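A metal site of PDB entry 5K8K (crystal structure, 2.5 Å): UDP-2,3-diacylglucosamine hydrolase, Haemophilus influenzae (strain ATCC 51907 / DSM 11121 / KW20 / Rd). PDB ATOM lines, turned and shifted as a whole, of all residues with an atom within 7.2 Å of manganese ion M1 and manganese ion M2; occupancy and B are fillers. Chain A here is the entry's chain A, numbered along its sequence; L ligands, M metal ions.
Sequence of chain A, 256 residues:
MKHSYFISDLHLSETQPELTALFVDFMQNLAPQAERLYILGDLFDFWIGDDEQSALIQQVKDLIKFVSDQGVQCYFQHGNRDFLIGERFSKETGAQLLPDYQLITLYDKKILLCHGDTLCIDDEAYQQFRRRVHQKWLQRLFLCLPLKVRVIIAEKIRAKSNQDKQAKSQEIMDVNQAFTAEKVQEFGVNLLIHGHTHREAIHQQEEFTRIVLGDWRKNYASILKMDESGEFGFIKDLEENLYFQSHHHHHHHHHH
N of His 196 sits at hydrogen-bond distance from OD2 of Asp 9. A ring nitrogen (NE2) of His 198 lies close to the backbone carbonyl oxygen (O) of His 196 (3.2 Å). N of Arg 81 lies within hydrogen-bond range of OD1 of Asp 42 (3.0 Å). The backbone carbonyl oxygen (O) of Asp 42 sits at hydrogen-bond distance from the backbone NH (N) of Leu 10 (2.9 Å). The side-chain hydroxyl (OG) of Ser 8 lies within hydrogen-bond range of the side-chain carboxylate (OD2) of Asp 9. The backbone NH of Gly 195 sits at hydrogen-bond distance from the backbone carbonyl oxygen of His 115. O of Leu 40 sits at hydrogen-bond distance from ND1 of His 115. The side-chain carboxylate (OD2) of Asp 215 is in hydrogen-bond range of a ring nitrogen (ND1) of His 198 (2.6 Å).
Manganese ion M1 is bound by OD1 of Asn 80 (2.0 Å), ND1 of His 196 (2.1 Å), OD2 of Asp 42 (2.1 Å) and NE2 of His 115 (2.3 Å). Manganese ion M1 has four donor atoms within binding distance.
Manganese ion M2 is bound by OD1 of Asp 9, 2.2 Å away. NE2 of His 11 binds manganese ion M2, at 2.3 Å. The side-chain carboxylate (OD2) of Asp 42 binds manganese ion M2, at 2.3 Å.
The nearest printed residue that does not touch manganese ion M1 is His 11 (5.3 Å).
ND2 of Asn 80 is in hydrogen-bond range of O3 of the ligand, at 3.0 Å. NE2 of His 196 is in hydrogen-bond range of O8 of the ligand, at 3.1 Å. The guanidinium group of Arg 81 is in salt-bridge range of an oxygen (O3) of the ligand, 2.7 Å away.
Residues that only touch manganese ion M2: His 198 (3.5 Å). Within 4 Å of manganese ion M2: Asp 9, His 11, Asp 42 and His 198.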
ATOM      1  N   SER A   8      24.000  -3.303  -6.412  1.00  0.00           N
ATOM      2  CA  SER A   8      24.247  -1.972  -6.923  1.00  0.00           C
ATOM      3  C   SER A   8      24.752  -1.102  -5.778  1.00  0.00           C
ATOM      4  O   SER A   8      24.838  -1.546  -4.631  1.00  0.00           O
ATOM      5  CB  SER A   8      22.989  -1.355  -7.542  1.00  0.00           C
ATOM      6  OG  SER A   8      22.020  -1.078  -6.551  1.00  0.00           O
ATOM      7  N   ASP A   9      25.099   0.136  -6.117  1.00  0.00           N
ATOM      8  CA  ASP A   9      25.403   1.186  -5.141  1.00  0.00           C
ATOM      9  C   ASP A   9      26.507   0.769  -4.173  1.00  0.00           C
ATOM     10  O   ASP A   9      26.408   0.934  -2.947  1.00  0.00           O
ATOM     11  CB  ASP A   9      24.142   1.616  -4.385  1.00  0.00           C
ATOM     12  CG  ASP A   9      23.238   2.490  -5.224  1.00  0.00           C
ATOM     13  OD1 ASP A   9      23.470   3.718  -5.279  1.00  0.00           O
ATOM     14  OD2 ASP A   9      22.290   1.939  -5.837  1.00  0.00           O
ATOM     15  N   LEU A  10      27.586   0.236  -4.736  1.00  0.00           N
ATOM     16  CA  LEU A  10      28.773  -0.099  -3.960  1.00  0.00           C
ATOM     17  C   LEU A  10      29.700   1.102  -3.790  1.00  0.00           C
ATOM     18  O   LEU A  10      30.388   1.196  -2.772  1.00  0.00           O
ATOM     19  CB  LEU A  10      29.527  -1.255  -4.626  1.00  0.00           C
ATOM     20  CG  LEU A  10      28.765  -2.576  -4.768  1.00  0.00           C
ATOM     21  CD1 LEU A  10      27.940  -2.636  -6.058  1.00  0.00           C
ATOM     22  CD2 LEU A  10      29.719  -3.769  -4.679  1.00  0.00           C
ATOM     23  N   HIS A  11      29.721   2.002  -4.770  1.00  0.00           N
ATOM     24  CA  HIS A  11      30.591   3.178  -4.795  1.00  0.00           C
ATOM     25  C   HIS A  11      32.007   2.820  -4.312  1.00  0.00           C
ATOM     26  O   HIS A  11      32.520   3.358  -3.334  1.00  0.00           O
ATOM     27  CB  HIS A  11      30.019   4.322  -3.965  1.00  0.00           C
ATOM     28  CG  HIS A  11      28.522   4.444  -4.027  1.00  0.00           C
ATOM     29  ND1 HIS A  11      27.691   3.809  -3.131  1.00  0.00           N
ATOM     30  CD2 HIS A  11      27.714   5.127  -4.869  1.00  0.00           C
ATOM     31  CE1 HIS A  11      26.433   4.097  -3.417  1.00  0.00           C
ATOM     32  NE2 HIS A  11      26.417   4.892  -4.474  1.00  0.00           N
ATOM     33  N   LEU A  40      23.458  -3.106 -11.058  1.00  0.00           N
ATOM     34  CA  LEU A  40      22.538  -2.060 -11.495  1.00  0.00           C
ATOM     35  C   LEU A  40      23.030  -0.670 -11.102  1.00  0.00           C
ATOM     36  O   LEU A  40      22.335   0.115 -10.464  1.00  0.00           O
ATOM     37  CB  LEU A  40      21.140  -2.327 -10.932  1.00  0.00           C
ATOM     38  CG  LEU A  40      20.562  -3.733 -11.099  1.00  0.00           C
ATOM     39  CD1 LEU A  40      19.136  -3.745 -10.576  1.00  0.00           C
ATOM     40  CD2 LEU A  40      20.613  -4.199 -12.547  1.00  0.00           C
ATOM     41  N   GLY A  41      24.246  -0.351 -11.531  1.00  0.00           N
ATOM     42  CA  GLY A  41      24.758   1.004 -11.442  1.00  0.00           C
ATOM     43  C   GLY A  41      25.497   1.293 -10.159  1.00  0.00           C
ATOM     44  O   GLY A  41      25.409   0.573  -9.161  1.00  0.00           O
ATOM     45  N   ASP A  42      26.227   2.408 -10.189  1.00  0.00           N
ATOM     46  CA  ASP A  42      27.012   2.879  -9.042  1.00  0.00           C
ATOM     47  C   ASP A  42      27.918   1.776  -8.504  1.00  0.00           C
ATOM     48  O   ASP A  42      27.994   1.535  -7.293  1.00  0.00           O
ATOM     49  CB  ASP A  42      26.110   3.457  -7.946  1.00  0.00           C
ATOM     50  CG  ASP A  42      25.351   4.687  -8.401  1.00  0.00           C
ATOM     51  OD1 ASP A  42      25.666   5.207  -9.484  1.00  0.00           O
ATOM     52  OD2 ASP A  42      24.450   5.154  -7.668  1.00  0.00           O
ATOM     53  N   PHE A  44      31.241   2.020  -9.094  1.00  0.00           N
ATOM     54  CA  PHE A  44      32.337   2.869  -8.658  1.00  0.00           C
ATOM     55  C   PHE A  44      31.801   4.153  -8.021  1.00  0.00           C
ATOM     56  O   PHE A  44      30.682   4.583  -8.265  1.00  0.00           O
ATOM     57  CB  PHE A  44      33.243   3.234  -9.832  1.00  0.00           C
ATOM     58  CG  PHE A  44      33.960   2.053 -10.435  1.00  0.00           C
ATOM     59  CD1 PHE A  44      35.086   1.524  -9.821  1.00  0.00           C
ATOM     60  CD2 PHE A  44      33.513   1.489 -11.614  1.00  0.00           C
ATOM     61  CE1 PHE A  44      35.747   0.446 -10.391  1.00  0.00           C
ATOM     62  CE2 PHE A  44      34.174   0.411 -12.183  1.00  0.00           C
ATOM     63  CZ  PHE A  44      35.290  -0.115 -11.570  1.00  0.00           C
ATOM     64  N   GLY A  79      24.679   3.621 -13.614  1.00  0.00           N
ATOM     65  CA  GLY A  79      24.186   4.462 -12.554  1.00  0.00           C
ATOM     66  C   GLY A  79      24.466   5.921 -12.864  1.00  0.00           C
ATOM     67  O   GLY A  79      24.970   6.288 -13.926  1.00  0.00           O
ATOM     68  N   ASN A  80      24.128   6.766 -11.896  1.00  0.00           N
ATOM     69  CA  ASN A  80      24.452   8.190 -11.977  1.00  0.00           C
ATOM     70  C   ASN A  80      25.929   8.474 -11.705  1.00  0.00           C
ATOM     71  O   ASN A  80      26.452   9.471 -12.203  1.00  0.00           O
ATOM     72  CB  ASN A  80      23.560   8.969 -11.000  1.00  0.00           C
ATOM     73  CG  ASN A  80      23.595   8.404  -9.589  1.00  0.00           C
ATOM     74  OD1 ASN A  80      23.017   7.352  -9.317  1.00  0.00           O
ATOM     75  ND2 ASN A  80      24.254   9.111  -8.686  1.00  0.00           N
ATOM     76  N   ARG A  81      26.608   7.608 -10.953  1.00  0.00           N
ATOM     77  CA  ARG A  81      28.026   7.823 -10.683  1.00  0.00           C
ATOM     78  C   ARG A  81      28.919   7.334 -11.813  1.00  0.00           C
ATOM     79  O   ARG A  81      30.032   7.851 -11.979  1.00  0.00           O
ATOM     80  CB  ARG A  81      28.438   7.120  -9.387  1.00  0.00           C
ATOM     81  CG  ARG A  81      27.648   7.526  -8.170  1.00  0.00           C
ATOM     82  CD  ARG A  81      28.080   8.882  -7.637  1.00  0.00           C
ATOM     83  NE  ARG A  81      27.519   9.095  -6.304  1.00  0.00           N
ATOM     84  CZ  ARG A  81      28.080   8.652  -5.190  1.00  0.00           C
ATOM     85  NH1 ARG A  81      29.233   7.995  -5.230  1.00  0.00           N
ATOM     86  NH2 ARG A  81      27.500   8.873  -4.018  1.00  0.00           N
ATOM     87  N   HIS A 115      18.224   1.585 -12.735  1.00  0.00           N
ATOM     88  CA  HIS A 115      19.057   2.042 -11.633  1.00  0.00           C
ATOM     89  C   HIS A 115      18.210   2.629 -10.516  1.00  0.00           C
ATOM     90  O   HIS A 115      18.477   2.370  -9.333  1.00  0.00           O
ATOM     91  CB  HIS A 115      20.080   3.059 -12.120  1.00  0.00           C
ATOM     92  CG  HIS A 115      20.977   3.564 -11.030  1.00  0.00           C
ATOM     93  ND1 HIS A 115      21.691   2.715 -10.212  1.00  0.00           N
ATOM     94  CD2 HIS A 115      21.246   4.810 -10.598  1.00  0.00           C
ATOM     95  CE1 HIS A 115      22.369   3.415  -9.332  1.00  0.00           C
ATOM     96  NE2 HIS A 115      22.119   4.700  -9.544  1.00  0.00           N
ATOM     97  N   GLY A 116      17.189   3.405 -10.853  1.00  0.00           N
ATOM     98  CA  GLY A 116      16.311   4.036  -9.880  1.00  0.00           C
ATOM     99  C   GLY A 116      16.287   5.551  -9.937  1.00  0.00           C
ATOM    100  O   GLY A 116      15.350   6.158  -9.410  1.00  0.00           O
ATOM    101  N   ASP A 117      17.292   6.180 -10.558  1.00  0.00           N
ATOM    102  CA  ASP A 117      17.336   7.640 -10.619  1.00  0.00           C
ATOM    103  C   ASP A 117      16.338   8.227 -11.612  1.00  0.00           C
ATOM    104  O   ASP A 117      15.908   9.369 -11.450  1.00  0.00           O
ATOM    105  CB  ASP A 117      18.746   8.111 -10.961  1.00  0.00           C
ATOM    106  CG  ASP A 117      19.162   7.738 -12.372  1.00  0.00           C
ATOM    107  OD1 ASP A 117      18.937   6.579 -12.776  1.00  0.00           O
ATOM    108  OD2 ASP A 117      19.713   8.605 -13.067  1.00  0.00           O
ATOM    109  N   TYR A 126      18.043  17.400 -10.286  1.00  0.00           N
ATOM    110  CA  TYR A 126      18.799  16.250 -10.751  1.00  0.00           C
ATOM    111  C   TYR A 126      18.411  15.879 -12.188  1.00  0.00           C
ATOM    112  O   TYR A 126      19.292  15.621 -13.017  1.00  0.00           O
ATOM    113  CB  TYR A 126      18.595  15.039  -9.842  1.00  0.00           C
ATOM    114  CG  TYR A 126      19.183  13.797 -10.464  1.00  0.00           C
ATOM    115  CD1 TYR A 126      20.563  13.664 -10.619  1.00  0.00           C
ATOM    116  CD2 TYR A 126      18.373  12.776 -10.951  1.00  0.00           C
ATOM    117  CE1 TYR A 126      21.115  12.562 -11.218  1.00  0.00           C
ATOM    118  CE2 TYR A 126      18.929  11.650 -11.549  1.00  0.00           C
ATOM    119  CZ  TYR A 126      20.298  11.557 -11.678  1.00  0.00           C
ATOM    120  OH  TYR A 126      20.869  10.446 -12.264  1.00  0.00           O
ATOM    121  N   GLY A 195      18.102   0.320  -7.592  1.00  0.00           N
ATOM    122  CA  GLY A 195      18.939   0.794  -6.522  1.00  0.00           C
ATOM    123  C   GLY A 195      18.830   2.302  -6.336  1.00  0.00           C
ATOM    124  O   GLY A 195      17.718   2.837  -6.328  1.00  0.00           O
ATOM    125  N   HIS A 196      19.981   2.965  -6.186  1.00  0.00           N
ATOM    126  CA  HIS A 196      20.126   4.416  -6.153  1.00  0.00           C
ATOM    127  C   HIS A 196      19.599   5.081  -4.882  1.00  0.00           C
ATOM    128  O   HIS A 196      20.269   5.956  -4.321  1.00  0.00           O
ATOM    129  CB  HIS A 196      19.462   5.062  -7.372  1.00  0.00           C
ATOM    130  CG  HIS A 196      19.585   6.549  -7.412  1.00  0.00           C
ATOM    131  ND1 HIS A 196      20.752   7.197  -7.780  1.00  0.00           N
ATOM    132  CD2 HIS A 196      18.692   7.532  -7.136  1.00  0.00           C
ATOM    133  CE1 HIS A 196      20.569   8.498  -7.725  1.00  0.00           C
ATOM    134  NE2 HIS A 196      19.319   8.731  -7.334  1.00  0.00           N
ATOM    135  N   THR A 197      18.410   4.706  -4.415  1.00  0.00           N
ATOM    136  CA  THR A 197      17.799   5.413  -3.292  1.00  0.00           C
ATOM    137  C   THR A 197      18.379   4.998  -1.933  1.00  0.00           C
ATOM    138  O   THR A 197      17.870   5.458  -0.909  1.00  0.00           O
ATOM    139  CB  THR A 197      16.275   5.226  -3.289  1.00  0.00           C
ATOM    140  OG1 THR A 197      15.957   3.822  -3.254  1.00  0.00           O
ATOM    141  CG2 THR A 197      15.658   5.855  -4.517  1.00  0.00           C
ATOM    142  N   HIS A 198      19.397   4.137  -1.915  1.00  0.00           N
ATOM    143  CA  HIS A 198      20.215   3.852  -0.738  1.00  0.00           C
ATOM    144  C   HIS A 198      19.497   3.010   0.321  1.00  0.00           C
ATOM    145  O   HIS A 198      20.150   2.328   1.116  1.00  0.00           O
ATOM    146  CB  HIS A 198      20.717   5.157  -0.096  1.00  0.00           C
ATOM    147  CG  HIS A 198      21.331   6.113  -1.063  1.00  0.00           C
ATOM    148  ND1 HIS A 198      22.423   5.794  -1.844  1.00  0.00           N
ATOM    149  CD2 HIS A 198      21.020   7.401  -1.360  1.00  0.00           C
ATOM    150  CE1 HIS A 198      22.742   6.844  -2.592  1.00  0.00           C
ATOM    151  NE2 HIS A 198      21.909   7.821  -2.321  1.00  0.00           N
ATOM    152  N   ASP A 215      22.728   0.601  -0.300  1.00  0.00           N
ATOM    153  CA  ASP A 215      24.149   0.909  -0.364  1.00  0.00           C
ATOM    154  C   ASP A 215      24.958  -0.132   0.406  1.00  0.00           C
ATOM    155  O   ASP A 215      24.481  -0.716   1.385  1.00  0.00           O
ATOM    156  CB  ASP A 215      24.442   2.288   0.211  1.00  0.00           C
ATOM    157  CG  ASP A 215      23.809   3.413  -0.582  1.00  0.00           C
ATOM    158  OD1 ASP A 215      23.342   3.176  -1.714  1.00  0.00           O
ATOM    159  OD2 ASP A 215      23.794   4.555  -0.067  1.00  0.00           O
HETATM  160  O1  LIG L   1      23.366   9.429  -5.107  1.00  0.00           O
HETATM  161  P1  LIG L   1      24.193  10.686  -5.215  1.00  0.00           P
HETATM  162  O2  LIG L   1      24.824  10.955  -3.871  1.00  0.00           O
HETATM  163  O3  LIG L   1      25.266  10.533  -6.274  1.00  0.00           O
HETATM  164  O4  LIG L   1      23.226  11.914  -5.685  1.00  0.00           O
HETATM  165  C1  LIG L   1      22.486  11.695  -6.823  1.00  0.00           C
HETATM  166  C2  LIG L   1      22.544  12.941  -7.695  1.00  0.00           C
HETATM  167  N1  LIG L   1      23.960  13.313  -7.918  1.00  0.00           N
HETATM  168  C3  LIG L   1      24.587  13.117  -9.212  1.00  0.00           C
HETATM  169  C4  LIG L   1      26.044  13.525  -9.436  1.00  0.00           C
HETATM  170  C5  LIG L   1      26.978  12.334  -9.311  1.00  0.00           C
HETATM  171  O5  LIG L   1      27.095  11.972  -7.962  1.00  0.00           O
HETATM  172  C6  LIG L   1      28.346  12.767  -9.844  1.00  0.00           C
HETATM  173  C7  LIG L   1      29.052  11.582 -10.478  1.00  0.00           C
HETATM  174  C8  LIG L   1      29.471  11.943 -11.901  1.00  0.00           C
HETATM  175  C9  LIG L   1      30.957  12.302 -11.887  1.00  0.00           C
HETATM  176  C10 LIG L   1      31.491  12.309 -13.321  1.00  0.00           C
HETATM  177  C11 LIG L   1      30.579  13.151 -14.199  1.00  0.00           C
HETATM  178  C12 LIG L   1      31.114  13.163 -15.624  1.00  0.00           C
HETATM  179  C13 LIG L   1      30.568  14.383 -16.354  1.00  0.00           C
HETATM  180  C14 LIG L   1      30.512  14.064 -17.842  1.00  0.00           C
HETATM  181  C15 LIG L   1      29.748  15.160 -18.578  1.00  0.00           C
HETATM  182  C16 LIG L   1      29.442  14.667 -19.985  1.00  0.00           C
HETATM  183  O6  LIG L   1      23.969  12.649 -10.110  1.00  0.00           O
HETATM  184  C17 LIG L   1      21.806  14.082  -7.068  1.00  0.00           C
HETATM  185  C18 LIG L   1      20.426  13.687  -6.702  1.00  0.00           C
HETATM  186  C19 LIG L   1      20.453  12.493  -5.743  1.00  0.00           C
HETATM  187  O7  LIG L   1      21.108  11.352  -6.427  1.00  0.00           O
HETATM  188  C20 LIG L   1      19.066  12.071  -5.407  1.00  0.00           C
HETATM  189  O8  LIG L   1      18.414  11.635  -6.557  1.00  0.00           O
HETATM  190  O9  LIG L   1      19.834  14.834  -6.064  1.00  0.00           O
HETATM  191  O10 LIG L   1      21.709  15.203  -8.002  1.00  0.00           O
HETATM  192  C21 LIG L   1      22.482  16.324  -7.688  1.00  0.00           C
HETATM  193  O11 LIG L   1      22.683  16.612  -6.546  1.00  0.00           O
HETATM  194  C22 LIG L   1      23.064  17.196  -8.800  1.00  0.00           C
HETATM  195  C23 LIG L   1      22.966  18.664  -8.389  1.00  0.00           C
HETATM  196  O12 LIG L   1      21.655  18.938  -7.953  1.00  0.00           O
HETATM  197  C24 LIG L   1      23.319  19.573  -9.557  1.00  0.00           C
HETATM  198  C25 LIG L   1      24.629  19.130 -10.189  1.00  0.00           C
HETATM  199  C26 LIG L   1      25.303  20.317 -10.865  1.00  0.00           C
HETATM  200  C27 LIG L   1      26.817  20.103 -10.916  1.00  0.00           C
HETATM  201  C28 LIG L   1      27.440  20.817 -12.121  1.00  0.00           C
HETATM  202  C29 LIG L   1      26.422  20.928 -13.258  1.00  0.00           C
HETATM  203  C30 LIG L   1      27.149  21.320 -14.548  1.00  0.00           C
HETATM  204  C31 LIG L   1      26.706  20.411 -15.692  1.00  0.00           C
HETATM  205  C32 LIG L   1      27.949  19.751 -16.279  1.00  0.00           C
HETATM  206  C33 LIG L   1      27.828  19.618 -17.799  1.00  0.00           C
HETATM  207  C34 LIG L   1      29.215  19.401 -18.390  1.00  0.00           C
HETATM  208 MN    MN M   1      22.543   6.132  -7.796  1.00  0.00          MN
HETATM  209 MN    MN M   2      24.422   5.660  -5.390  1.00  0.00          MN
